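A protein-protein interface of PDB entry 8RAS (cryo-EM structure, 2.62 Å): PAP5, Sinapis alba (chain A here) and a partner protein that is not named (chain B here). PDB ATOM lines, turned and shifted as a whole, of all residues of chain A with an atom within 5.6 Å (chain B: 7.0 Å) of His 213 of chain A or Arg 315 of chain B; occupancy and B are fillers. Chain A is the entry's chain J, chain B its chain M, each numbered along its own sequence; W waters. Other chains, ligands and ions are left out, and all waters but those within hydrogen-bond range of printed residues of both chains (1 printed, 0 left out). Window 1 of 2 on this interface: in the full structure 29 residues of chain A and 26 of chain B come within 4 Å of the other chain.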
ATOM      1  N   PHE A 203      33.417 -30.390 -15.573  1.00  0.00           N
ATOM      2  CA  PHE A 203      32.624 -29.352 -16.209  1.00  0.00           C
ATOM      3  C   PHE A 203      32.940 -29.291 -17.704  1.00  0.00           C
ATOM      4  O   PHE A 203      33.906 -29.882 -18.190  1.00  0.00           O
ATOM      5  CB  PHE A 203      32.883 -27.999 -15.548  1.00  0.00           C
ATOM      6  CG  PHE A 203      31.659 -27.136 -15.430  1.00  0.00           C
ATOM      7  CD1 PHE A 203      30.807 -27.265 -14.348  1.00  0.00           C
ATOM      8  CD2 PHE A 203      31.365 -26.191 -16.398  1.00  0.00           C
ATOM      9  CE1 PHE A 203      29.684 -26.472 -14.237  1.00  0.00           C
ATOM     10  CE2 PHE A 203      30.243 -25.396 -16.290  1.00  0.00           C
ATOM     11  CZ  PHE A 203      29.403 -25.537 -15.208  1.00  0.00           C
ATOM     12  N   ASP A 206      29.827 -32.409 -18.453  1.00  0.00           N
ATOM     13  CA  ASP A 206      28.567 -32.618 -17.751  1.00  0.00           C
ATOM     14  C   ASP A 206      27.533 -31.588 -18.179  1.00  0.00           C
ATOM     15  O   ASP A 206      26.346 -31.904 -18.309  1.00  0.00           O
ATOM     16  CB  ASP A 206      28.790 -32.554 -16.240  1.00  0.00           C
ATOM     17  CG  ASP A 206      29.493 -33.781 -15.704  1.00  0.00           C
ATOM     18  OD1 ASP A 206      29.501 -34.816 -16.400  1.00  0.00           O
ATOM     19  OD2 ASP A 206      30.039 -33.710 -14.584  1.00  0.00           O
ATOM     20  N   LYS A 207      27.966 -30.343 -18.390  1.00  0.00           N
ATOM     21  CA  LYS A 207      27.050 -29.312 -18.862  1.00  0.00           C
ATOM     22  C   LYS A 207      26.550 -29.618 -20.268  1.00  0.00           C
ATOM     23  O   LYS A 207      25.376 -29.390 -20.578  1.00  0.00           O
ATOM     24  CB  LYS A 207      27.730 -27.944 -18.817  1.00  0.00           C
ATOM     25  CG  LYS A 207      26.818 -26.798 -19.213  1.00  0.00           C
ATOM     26  CD  LYS A 207      27.516 -25.460 -19.084  1.00  0.00           C
ATOM     27  CE  LYS A 207      26.605 -24.331 -19.531  1.00  0.00           C
ATOM     28  NZ  LYS A 207      27.249 -23.000 -19.368  1.00  0.00           N
ATOM     29  N   GLY A 210      24.216 -32.784 -20.084  1.00  0.00           N
ATOM     30  CA  GLY A 210      23.065 -32.680 -19.214  1.00  0.00           C
ATOM     31  C   GLY A 210      23.186 -33.434 -17.912  1.00  0.00           C
ATOM     32  O   GLY A 210      22.190 -33.561 -17.193  1.00  0.00           O
ATOM     33  N   ARG A 211      24.372 -33.944 -17.590  1.00  0.00           N
ATOM     34  CA  ARG A 211      24.590 -34.624 -16.328  1.00  0.00           C
ATOM     35  C   ARG A 211      24.582 -33.614 -15.183  1.00  0.00           C
ATOM     36  O   ARG A 211      24.828 -32.425 -15.392  1.00  0.00           O
ATOM     37  CB  ARG A 211      25.910 -35.386 -16.361  1.00  0.00           C
ATOM     38  CG  ARG A 211      25.875 -36.630 -17.228  1.00  0.00           C
ATOM     39  CD  ARG A 211      27.069 -37.524 -16.959  1.00  0.00           C
ATOM     40  NE  ARG A 211      28.327 -36.874 -17.303  1.00  0.00           N
ATOM     41  CZ  ARG A 211      29.280 -37.428 -18.040  1.00  0.00           C
ATOM     42  NH1 ARG A 211      29.153 -38.651 -18.527  1.00  0.00           N
ATOM     43  NH2 ARG A 211      30.388 -36.738 -18.292  1.00  0.00           N
ATOM     44  N   PRO A 212      24.275 -34.061 -13.964  1.00  0.00           N
ATOM     45  CA  PRO A 212      24.208 -33.126 -12.834  1.00  0.00           C
ATOM     46  C   PRO A 212      25.516 -32.373 -12.637  1.00  0.00           C
ATOM     47  O   PRO A 212      26.586 -32.969 -12.503  1.00  0.00           O
ATOM     48  CB  PRO A 212      23.891 -34.037 -11.645  1.00  0.00           C
ATOM     49  CG  PRO A 212      23.188 -35.192 -12.242  1.00  0.00           C
ATOM     50  CD  PRO A 212      23.819 -35.409 -13.587  1.00  0.00           C
ATOM     51  N   HIS A 213      25.417 -31.047 -12.621  1.00  0.00           N
ATOM     52  CA  HIS A 213      26.575 -30.174 -12.509  1.00  0.00           C
ATOM     53  C   HIS A 213      26.119 -28.850 -11.918  1.00  0.00           C
ATOM     54  O   HIS A 213      24.942 -28.489 -12.033  1.00  0.00           O
ATOM     55  CB  HIS A 213      27.238 -29.951 -13.878  1.00  0.00           C
ATOM     56  CG  HIS A 213      26.413 -29.128 -14.819  1.00  0.00           C
ATOM     57  ND1 HIS A 213      26.527 -27.758 -14.905  1.00  0.00           N
ATOM     58  CD2 HIS A 213      25.458 -29.482 -15.709  1.00  0.00           C
ATOM     59  CE1 HIS A 213      25.679 -27.304 -15.809  1.00  0.00           C
ATOM     60  NE2 HIS A 213      25.018 -28.330 -16.313  1.00  0.00           N
ATOM     61  N   PRO A 214      27.018 -28.108 -11.272  1.00  0.00           N
ATOM     62  CA  PRO A 214      26.660 -26.767 -10.800  1.00  0.00           C
ATOM     63  C   PRO A 214      26.284 -25.852 -11.955  1.00  0.00           C
ATOM     64  O   PRO A 214      26.824 -25.952 -13.059  1.00  0.00           O
ATOM     65  CB  PRO A 214      27.935 -26.283 -10.099  1.00  0.00           C
ATOM     66  CG  PRO A 214      28.676 -27.521  -9.755  1.00  0.00           C
ATOM     67  CD  PRO A 214      28.362 -28.514 -10.827  1.00  0.00           C
ATOM     68  N   PHE A 215      25.332 -24.956 -11.690  1.00  0.00           N
ATOM     69  CA  PHE A 215      24.949 -23.972 -12.696  1.00  0.00           C
ATOM     70  C   PHE A 215      26.109 -23.041 -13.020  1.00  0.00           C
ATOM     71  O   PHE A 215      26.312 -22.670 -14.181  1.00  0.00           O
ATOM     72  CB  PHE A 215      23.735 -23.177 -12.217  1.00  0.00           C
ATOM     73  CG  PHE A 215      22.421 -23.767 -12.639  1.00  0.00           C
ATOM     74  CD1 PHE A 215      22.136 -23.966 -13.980  1.00  0.00           C
ATOM     75  CD2 PHE A 215      21.471 -24.120 -11.699  1.00  0.00           C
ATOM     76  CE1 PHE A 215      20.931 -24.507 -14.371  1.00  0.00           C
ATOM     77  CE2 PHE A 215      20.264 -24.661 -12.085  1.00  0.00           C
ATOM     78  CZ  PHE A 215      19.993 -24.855 -13.423  1.00  0.00           C
ATOM     79  N   LYS A 270      22.325 -35.455  -8.049  1.00  0.00           N
ATOM     80  CA  LYS A 270      23.106 -34.839  -6.988  1.00  0.00           C
ATOM     81  C   LYS A 270      22.839 -33.342  -6.978  1.00  0.00           C
ATOM     82  O   LYS A 270      22.756 -32.707  -8.033  1.00  0.00           O
ATOM     83  CB  LYS A 270      24.607 -35.121  -7.149  1.00  0.00           C
ATOM     84  CG  LYS A 270      25.225 -34.587  -8.423  1.00  0.00           C
ATOM     85  CD  LYS A 270      26.642 -35.098  -8.605  1.00  0.00           C
ATOM     86  CE  LYS A 270      26.657 -36.511  -9.160  1.00  0.00           C
ATOM     87  NZ  LYS A 270      28.018 -37.112  -9.100  1.00  0.00           N
ATOM     88  N   GLU B 309      18.401 -29.838 -31.555  1.00  0.00           N
ATOM     89  CA  GLU B 309      18.061 -28.418 -31.599  1.00  0.00           C
ATOM     90  C   GLU B 309      17.130 -28.041 -30.452  1.00  0.00           C
ATOM     91  O   GLU B 309      17.333 -27.020 -29.776  1.00  0.00           O
ATOM     92  CB  GLU B 309      17.422 -28.073 -32.943  1.00  0.00           C
ATOM     93  CG  GLU B 309      18.376 -28.146 -34.108  1.00  0.00           C
ATOM     94  CD  GLU B 309      19.471 -27.104 -34.038  1.00  0.00           C
ATOM     95  OE1 GLU B 309      19.199 -25.981 -33.562  1.00  0.00           O
ATOM     96  OE2 GLU B 309      20.605 -27.405 -34.463  1.00  0.00           O
ATOM     97  N   GLU B 310      16.105 -28.864 -30.216  1.00  0.00           N
ATOM     98  CA  GLU B 310      15.157 -28.579 -29.146  1.00  0.00           C
ATOM     99  C   GLU B 310      15.840 -28.583 -27.788  1.00  0.00           C
ATOM    100  O   GLU B 310      15.591 -27.701 -26.960  1.00  0.00           O
ATOM    101  CB  GLU B 310      14.017 -29.595 -29.173  1.00  0.00           C
ATOM    102  CG  GLU B 310      13.043 -29.409 -30.316  1.00  0.00           C
ATOM    103  CD  GLU B 310      12.003 -30.508 -30.373  1.00  0.00           C
ATOM    104  OE1 GLU B 310      12.258 -31.597 -29.820  1.00  0.00           O
ATOM    105  OE2 GLU B 310      10.931 -30.283 -30.972  1.00  0.00           O
ATOM    106  N   TRP B 311      16.709 -29.566 -27.543  1.00  0.00           N
ATOM    107  CA  TRP B 311      17.396 -29.650 -26.262  1.00  0.00           C
ATOM    108  C   TRP B 311      18.279 -28.438 -26.034  1.00  0.00           C
ATOM    109  O   TRP B 311      18.271 -27.855 -24.946  1.00  0.00           O
ATOM    110  CB  TRP B 311      18.221 -30.935 -26.192  1.00  0.00           C
ATOM    111  CG  TRP B 311      18.399 -31.453 -24.799  1.00  0.00           C
ATOM    112  CD1 TRP B 311      17.609 -32.357 -24.153  1.00  0.00           C
ATOM    113  CD2 TRP B 311      19.431 -31.093 -23.876  1.00  0.00           C
ATOM    114  NE1 TRP B 311      18.085 -32.585 -22.887  1.00  0.00           N
ATOM    115  CE2 TRP B 311      19.204 -31.819 -22.691  1.00  0.00           C
ATOM    116  CE3 TRP B 311      20.526 -30.227 -23.936  1.00  0.00           C
ATOM    117  CZ2 TRP B 311      20.031 -31.707 -21.578  1.00  0.00           C
ATOM    118  CZ3 TRP B 311      21.345 -30.118 -22.832  1.00  0.00           C
ATOM    119  CH2 TRP B 311      21.093 -30.854 -21.668  1.00  0.00           C
ATOM    120  N   THR B 312      19.034 -28.028 -27.054  1.00  0.00           N
ATOM    121  CA  THR B 312      19.901 -26.865 -26.900  1.00  0.00           C
ATOM    122  C   THR B 312      19.089 -25.611 -26.584  1.00  0.00           C
ATOM    123  O   THR B 312      19.365 -24.903 -25.600  1.00  0.00           O
ATOM    124  CB  THR B 312      20.735 -26.678 -28.168  1.00  0.00           C
ATOM    125  OG1 THR B 312      21.691 -27.740 -28.267  1.00  0.00           O
ATOM    126  CG2 THR B 312      21.468 -25.356 -28.144  1.00  0.00           C
ATOM    127  N   LYS B 313      18.063 -25.334 -27.395  1.00  0.00           N
ATOM    128  CA  LYS B 313      17.290 -24.112 -27.196  1.00  0.00           C
ATOM    129  C   LYS B 313      16.577 -24.117 -25.848  1.00  0.00           C
ATOM    130  O   LYS B 313      16.579 -23.107 -25.134  1.00  0.00           O
ATOM    131  CB  LYS B 313      16.289 -23.924 -28.333  1.00  0.00           C
ATOM    132  CG  LYS B 313      15.501 -22.627 -28.235  1.00  0.00           C
ATOM    133  CD  LYS B 313      14.645 -22.391 -29.464  1.00  0.00           C
ATOM    134  CE  LYS B 313      13.396 -23.250 -29.434  1.00  0.00           C
ATOM    135  NZ  LYS B 313      12.537 -22.930 -28.261  1.00  0.00           N
ATOM    136  N   THR B 314      15.973 -25.248 -25.476  1.00  0.00           N
ATOM    137  CA  THR B 314      15.250 -25.319 -24.213  1.00  0.00           C
ATOM    138  C   THR B 314      16.189 -25.253 -23.018  1.00  0.00           C
ATOM    139  O   THR B 314      15.820 -24.699 -21.980  1.00  0.00           O
ATOM    140  CB  THR B 314      14.416 -26.596 -24.159  1.00  0.00           C
ATOM    141  OG1 THR B 314      15.212 -27.699 -24.606  1.00  0.00           O
ATOM    142  CG2 THR B 314      13.196 -26.468 -25.050  1.00  0.00           C
ATOM    143  N   ARG B 315      17.399 -25.805 -23.137  1.00  0.00           N
ATOM    144  CA  ARG B 315      18.367 -25.699 -22.053  1.00  0.00           C
ATOM    145  C   ARG B 315      18.771 -24.251 -21.824  1.00  0.00           C
ATOM    146  O   ARG B 315      18.820 -23.785 -20.677  1.00  0.00           O
ATOM    147  CB  ARG B 315      19.587 -26.565 -22.366  1.00  0.00           C
ATOM    148  CG  ARG B 315      20.740 -26.415 -21.394  1.00  0.00           C
ATOM    149  CD  ARG B 315      20.535 -27.274 -20.160  1.00  0.00           C
ATOM    150  NE  ARG B 315      21.684 -27.236 -19.265  1.00  0.00           N
ATOM    151  CZ  ARG B 315      21.972 -26.228 -18.454  1.00  0.00           C
ATOM    152  NH1 ARG B 315      21.212 -25.148 -18.395  1.00  0.00           N
ATOM    153  NH2 ARG B 315      23.050 -26.307 -17.680  1.00  0.00           N
ATOM    154  N   GLU B 316      19.048 -23.512 -22.904  1.00  0.00           N
ATOM    155  CA  GLU B 316      19.366 -22.095 -22.729  1.00  0.00           C
ATOM    156  C   GLU B 316      18.180 -21.323 -22.161  1.00  0.00           C
ATOM    157  O   GLU B 316      18.354 -20.456 -21.295  1.00  0.00           O
ATOM    158  CB  GLU B 316      19.832 -21.468 -24.041  1.00  0.00           C
ATOM    159  CG  GLU B 316      21.291 -21.721 -24.357  1.00  0.00           C
ATOM    160  CD  GLU B 316      21.489 -22.890 -25.287  1.00  0.00           C
ATOM    161  OE1 GLU B 316      21.010 -22.807 -26.435  1.00  0.00           O
ATOM    162  OE2 GLU B 316      22.111 -23.892 -24.872  1.00  0.00           O
ATOM    163  N   ASP B 317      16.967 -21.619 -22.635  1.00  0.00           N
ATOM    164  CA  ASP B 317      15.789 -20.929 -22.118  1.00  0.00           C
ATOM    165  C   ASP B 317      15.597 -21.195 -20.630  1.00  0.00           C
ATOM    166  O   ASP B 317      15.291 -20.276 -19.861  1.00  0.00           O
ATOM    167  CB  ASP B 317      14.547 -21.354 -22.899  1.00  0.00           C
ATOM    168  CG  ASP B 317      14.383 -20.587 -24.192  1.00  0.00           C
ATOM    169  OD1 ASP B 317      15.325 -19.867 -24.582  1.00  0.00           O
ATOM    170  OD2 ASP B 317      13.309 -20.703 -24.819  1.00  0.00           O
ATOM    171  N   MET B 318      15.772 -22.448 -20.207  1.00  0.00           N
ATOM    172  CA  MET B 318      15.617 -22.788 -18.799  1.00  0.00           C
ATOM    173  C   MET B 318      16.683 -22.115 -17.948  1.00  0.00           C
ATOM    174  O   MET B 318      16.391 -21.641 -16.843  1.00  0.00           O
ATOM    175  CB  MET B 318      15.661 -24.304 -18.616  1.00  0.00           C
ATOM    176  CG  MET B 318      15.310 -24.765 -17.213  1.00  0.00           C
ATOM    177  SD  MET B 318      13.832 -23.964 -16.569  1.00  0.00           S
ATOM    178  CE  MET B 318      12.589 -25.173 -16.989  1.00  0.00           C
ATOM    179  N   GLU B 319      17.925 -22.064 -18.435  1.00  0.00           N
ATOM    180  CA  GLU B 319      18.964 -21.367 -17.684  1.00  0.00           C
ATOM    181  C   GLU B 319      18.648 -19.882 -17.559  1.00  0.00           C
ATOM    182  O   GLU B 319      18.890 -19.276 -16.509  1.00  0.00           O
ATOM    183  CB  GLU B 319      20.329 -21.573 -18.336  1.00  0.00           C
ATOM    184  CG  GLU B 319      21.488 -21.151 -17.450  1.00  0.00           C
ATOM    185  CD  GLU B 319      22.668 -22.092 -17.544  1.00  0.00           C
ATOM    186  OE1 GLU B 319      22.781 -22.805 -18.562  1.00  0.00           O
ATOM    187  OE2 GLU B 319      23.482 -22.120 -16.598  1.00  0.00           O
ATOM    188  N   LYS B 320      18.113 -19.276 -18.621  1.00  0.00           N
ATOM    189  CA  LYS B 320      17.734 -17.868 -18.547  1.00  0.00           C
ATOM    190  C   LYS B 320      16.598 -17.646 -17.555  1.00  0.00           C
ATOM    191  O   LYS B 320      16.590 -16.646 -16.827  1.00  0.00           O
ATOM    192  CB  LYS B 320      17.345 -17.352 -19.931  1.00  0.00           C
ATOM    193  CG  LYS B 320      18.526 -16.921 -20.780  1.00  0.00           C
ATOM    194  CD  LYS B 320      18.111 -16.650 -22.215  1.00  0.00           C
ATOM    195  CE  LYS B 320      19.318 -16.343 -23.085  1.00  0.00           C
ATOM    196  NZ  LYS B 320      18.944 -16.185 -24.516  1.00  0.00           N
ATOM    197  N   HIS B 321      15.624 -18.557 -17.520  1.00  0.00           N
ATOM    198  CA  HIS B 321      14.492 -18.393 -16.610  1.00  0.00           C
ATOM    199  C   HIS B 321      14.916 -18.550 -15.153  1.00  0.00           C
ATOM    200  O   HIS B 321      14.459 -17.796 -14.285  1.00  0.00           O
ATOM    201  CB  HIS B 321      13.392 -19.394 -16.956  1.00  0.00           C
ATOM    202  CG  HIS B 321      12.237 -19.373 -16.005  1.00  0.00           C
ATOM    203  ND1 HIS B 321      11.987 -20.394 -15.114  1.00  0.00           N
ATOM    204  CD2 HIS B 321      11.261 -18.456 -15.806  1.00  0.00           C
ATOM    205  CE1 HIS B 321      10.909 -20.107 -14.408  1.00  0.00           C
ATOM    206  NE2 HIS B 321      10.450 -18.936 -14.808  1.00  0.00           N
ATOM    207  N   PHE B 328      20.336 -19.228  -7.358  1.00  0.00           N
ATOM    208  CA  PHE B 328      20.799 -19.862  -8.588  1.00  0.00           C
ATOM    209  C   PHE B 328      22.288 -20.175  -8.537  1.00  0.00           C
ATOM    210  O   PHE B 328      22.731 -21.175  -9.112  1.00  0.00           O
ATOM    211  CB  PHE B 328      20.474 -18.955  -9.777  1.00  0.00           C
ATOM    212  CG  PHE B 328      20.983 -19.463 -11.095  1.00  0.00           C
ATOM    213  CD1 PHE B 328      20.231 -20.348 -11.848  1.00  0.00           C
ATOM    214  CD2 PHE B 328      22.201 -19.031 -11.597  1.00  0.00           C
ATOM    215  CE1 PHE B 328      20.690 -20.808 -13.064  1.00  0.00           C
ATOM    216  CE2 PHE B 328      22.666 -19.490 -12.812  1.00  0.00           C
ATOM    217  CZ  PHE B 328      21.909 -20.378 -13.547  1.00  0.00           C
ATOM    218  N   SER B 331      22.997 -23.584  -6.817  1.00  0.00           N
ATOM    219  CA  SER B 331      22.084 -24.605  -7.304  1.00  0.00           C
ATOM    220  C   SER B 331      22.767 -25.466  -8.357  1.00  0.00           C
ATOM    221  O   SER B 331      23.736 -25.054  -9.000  1.00  0.00           O
ATOM    222  CB  SER B 331      20.811 -23.980  -7.888  1.00  0.00           C
ATOM    223  OG  SER B 331      19.946 -23.541  -6.859  1.00  0.00           O
ATOM    224  N   ASN B 332      22.245 -26.676  -8.521  1.00  0.00           N
ATOM    225  CA  ASN B 332      22.745 -27.641  -9.487  1.00  0.00           C
ATOM    226  C   ASN B 332      21.743 -27.827 -10.618  1.00  0.00           C
ATOM    227  O   ASN B 332      20.536 -27.651 -10.438  1.00  0.00           O
ATOM    228  CB  ASN B 332      23.007 -28.999  -8.828  1.00  0.00           C
ATOM    229  CG  ASN B 332      24.477 -29.282  -8.634  1.00  0.00           C
ATOM    230  OD1 ASN B 332      25.276 -28.370  -8.448  1.00  0.00           O
ATOM    231  ND2 ASN B 332      24.842 -30.555  -8.675  1.00  0.00           N
ATOM    232  N   TRP B 333      22.260 -28.180 -11.788  1.00  0.00           N
ATOM    233  CA  TRP B 333      21.441 -28.726 -12.858  1.00  0.00           C
ATOM    234  C   TRP B 333      21.335 -30.236 -12.682  1.00  0.00           C
ATOM    235  O   TRP B 333      22.254 -30.881 -12.176  1.00  0.00           O
ATOM    236  CB  TRP B 333      22.033 -28.393 -14.229  1.00  0.00           C
ATOM    237  CG  TRP B 333      21.495 -29.246 -15.341  1.00  0.00           C
ATOM    238  CD1 TRP B 333      22.005 -30.431 -15.784  1.00  0.00           C
ATOM    239  CD2 TRP B 333      20.337 -28.986 -16.142  1.00  0.00           C
ATOM    240  NE1 TRP B 333      21.239 -30.923 -16.810  1.00  0.00           N
ATOM    241  CE2 TRP B 333      20.208 -30.054 -17.049  1.00  0.00           C
ATOM    242  CE3 TRP B 333      19.398 -27.951 -16.183  1.00  0.00           C
ATOM    243  CZ2 TRP B 333      19.181 -30.118 -17.985  1.00  0.00           C
ATOM    244  CZ3 TRP B 333      18.379 -28.019 -17.111  1.00  0.00           C
ATOM    245  CH2 TRP B 333      18.278 -29.094 -17.998  1.00  0.00           C
ATOM    246  N   PHE B 334      20.198 -30.793 -13.083  1.00  0.00           N
ATOM    247  CA  PHE B 334      20.022 -32.241 -13.067  1.00  0.00           C
ATOM    248  C   PHE B 334      18.907 -32.665 -14.015  1.00  0.00           C
ATOM    249  O   PHE B 334      18.152 -31.829 -14.507  1.00  0.00           O
ATOM    250  CB  PHE B 334      19.732 -32.743 -11.648  1.00  0.00           C
ATOM    251  CG  PHE B 334      18.607 -32.022 -10.966  1.00  0.00           C
ATOM    252  CD1 PHE B 334      17.297 -32.428 -11.148  1.00  0.00           C
ATOM    253  CD2 PHE B 334      18.859 -30.941 -10.142  1.00  0.00           C
ATOM    254  CE1 PHE B 334      16.265 -31.769 -10.527  1.00  0.00           C
ATOM    255  CE2 PHE B 334      17.829 -30.279  -9.518  1.00  0.00           C
ATOM    256  CZ  PHE B 334      16.532 -30.693  -9.711  1.00  0.00           C
HETATM  257  O   HOH W   1      23.457 -28.998 -18.562  1.00  0.00           O
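Water W1 lies within hydrogen-bond range of NE of Arg 315 of chain B (2.6 Å), O of Lys 207 of chain A (2.8 Å), NE2 of His 213 of chain A (2.8 Å) and NE1 of Trp 333 of chain B (3.4 Å).
Among the printed residues, pairs that only touch across the chains: Pro 212 of chain A with Trp 333 of chain B, Phe 215 of chain A with Asn 332 of chain B, Phe 215 of chain A with Phe 328 of chain B, His 213 of chain A with Asn 332 of chain B, Phe 215 of chain A with Glu 319 of chain B, Arg 211 of chain A with Trp 333 of chain B, Gly 210 of chain A with Trp 311 of chain B and Pro 214 of chain A with Ser 331 of chain B.
Of the 18 printed residues of chain B, 7 touch a printed residue of chain A. Hydrophobic or aromatic side chains of chain B that line the printed part of chain A: Trp 311, Phe 328 and Trp 333. Of the 10 printed residues of chain A, 7 touch a printed residue of chain B. Printed residues of chain A that touch a printed residue of chain B: Gly 210, Arg 211, Pro 212, His 213, Pro 214, Phe 215 and Lys 270. Hydrophobic or aromatic side chains of chain A that line the printed part of chain B: Pro 212, His 213, Pro 214 and Phe 215.
The guanidinium group (NH2) of Arg 315 of chain B sits at hydrogen-bond distance from a ring nitrogen (NE2) of His 213 of chain A (3.1 Å). The backbone carbonyl oxygen of Ser 331 of chain B lies within hydrogen-bond range of the backbone NH of Phe 215 of chain A, at 3.1 Å. The backbone carbonyl oxygen (O) of Lys 270 of chain A is in hydrogen-bond range of the side-chain amide nitrogen (ND2) of Asn 332 of chain B (3.1 Å). O of Gly 210 of chain A sits at hydrogen-bond distance from NE1 of Trp 333 of chain B (2.8 Å). N of Trp 333 of chain B is in hydrogen-bond range of O of His 213 of chain A, 2.7 Å away. The side-chain amide oxygen of Asn 332 of chain B lies close to the backbone nitrogen of Pro 214 of chain A (3.3 Å).
His 213 of chain A touches just these residues of chain B: Arg 315, Asn 332 and Trp 333. Of chain A, only His 213 comes within 4 Å of Arg 315 of chain B. Printed residues of chain B within 4 Å of Arg 211 of chain A: Trp 333. Printed residues of chain B within 4 Å of Gly 210 of chain A: Trp 311 (3.6 Å) and Trp 333 (2.8 Å). Printed residues of chain A within 4 Å of Phe 328 of chain B: Phe 215. Of the printed residues of chain B, Phe 215 of chain A touches Glu 319 (3.5 Å), Phe 328 (3.5 Å), Ser 331 (3.1 Å) and Asn 332 (3.4 Å). The nearest residue of chain B that does not touch His 213 of chain A is Ser 331 of chain B (4.7 Å). The nearest printed residue of chain A that does not touch Arg 315 of chain B is Phe 215 of chain A (4.1 Å).
The backbone carbonyl oxygen (O) of Trp 311 of chain B is in hydrogen-bond range of the side-chain hydroxyl (OG1) of Thr 314 of chain B (3.1 Å). OE1 of Glu 319 of chain B is in salt-bridge range of NH1 of Arg 315 of chain B (2.8 Å). NE of Arg 211 of chain A lies within salt-bridge range of OD1 of Asp 206 of chain A, 2.5 Å away.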
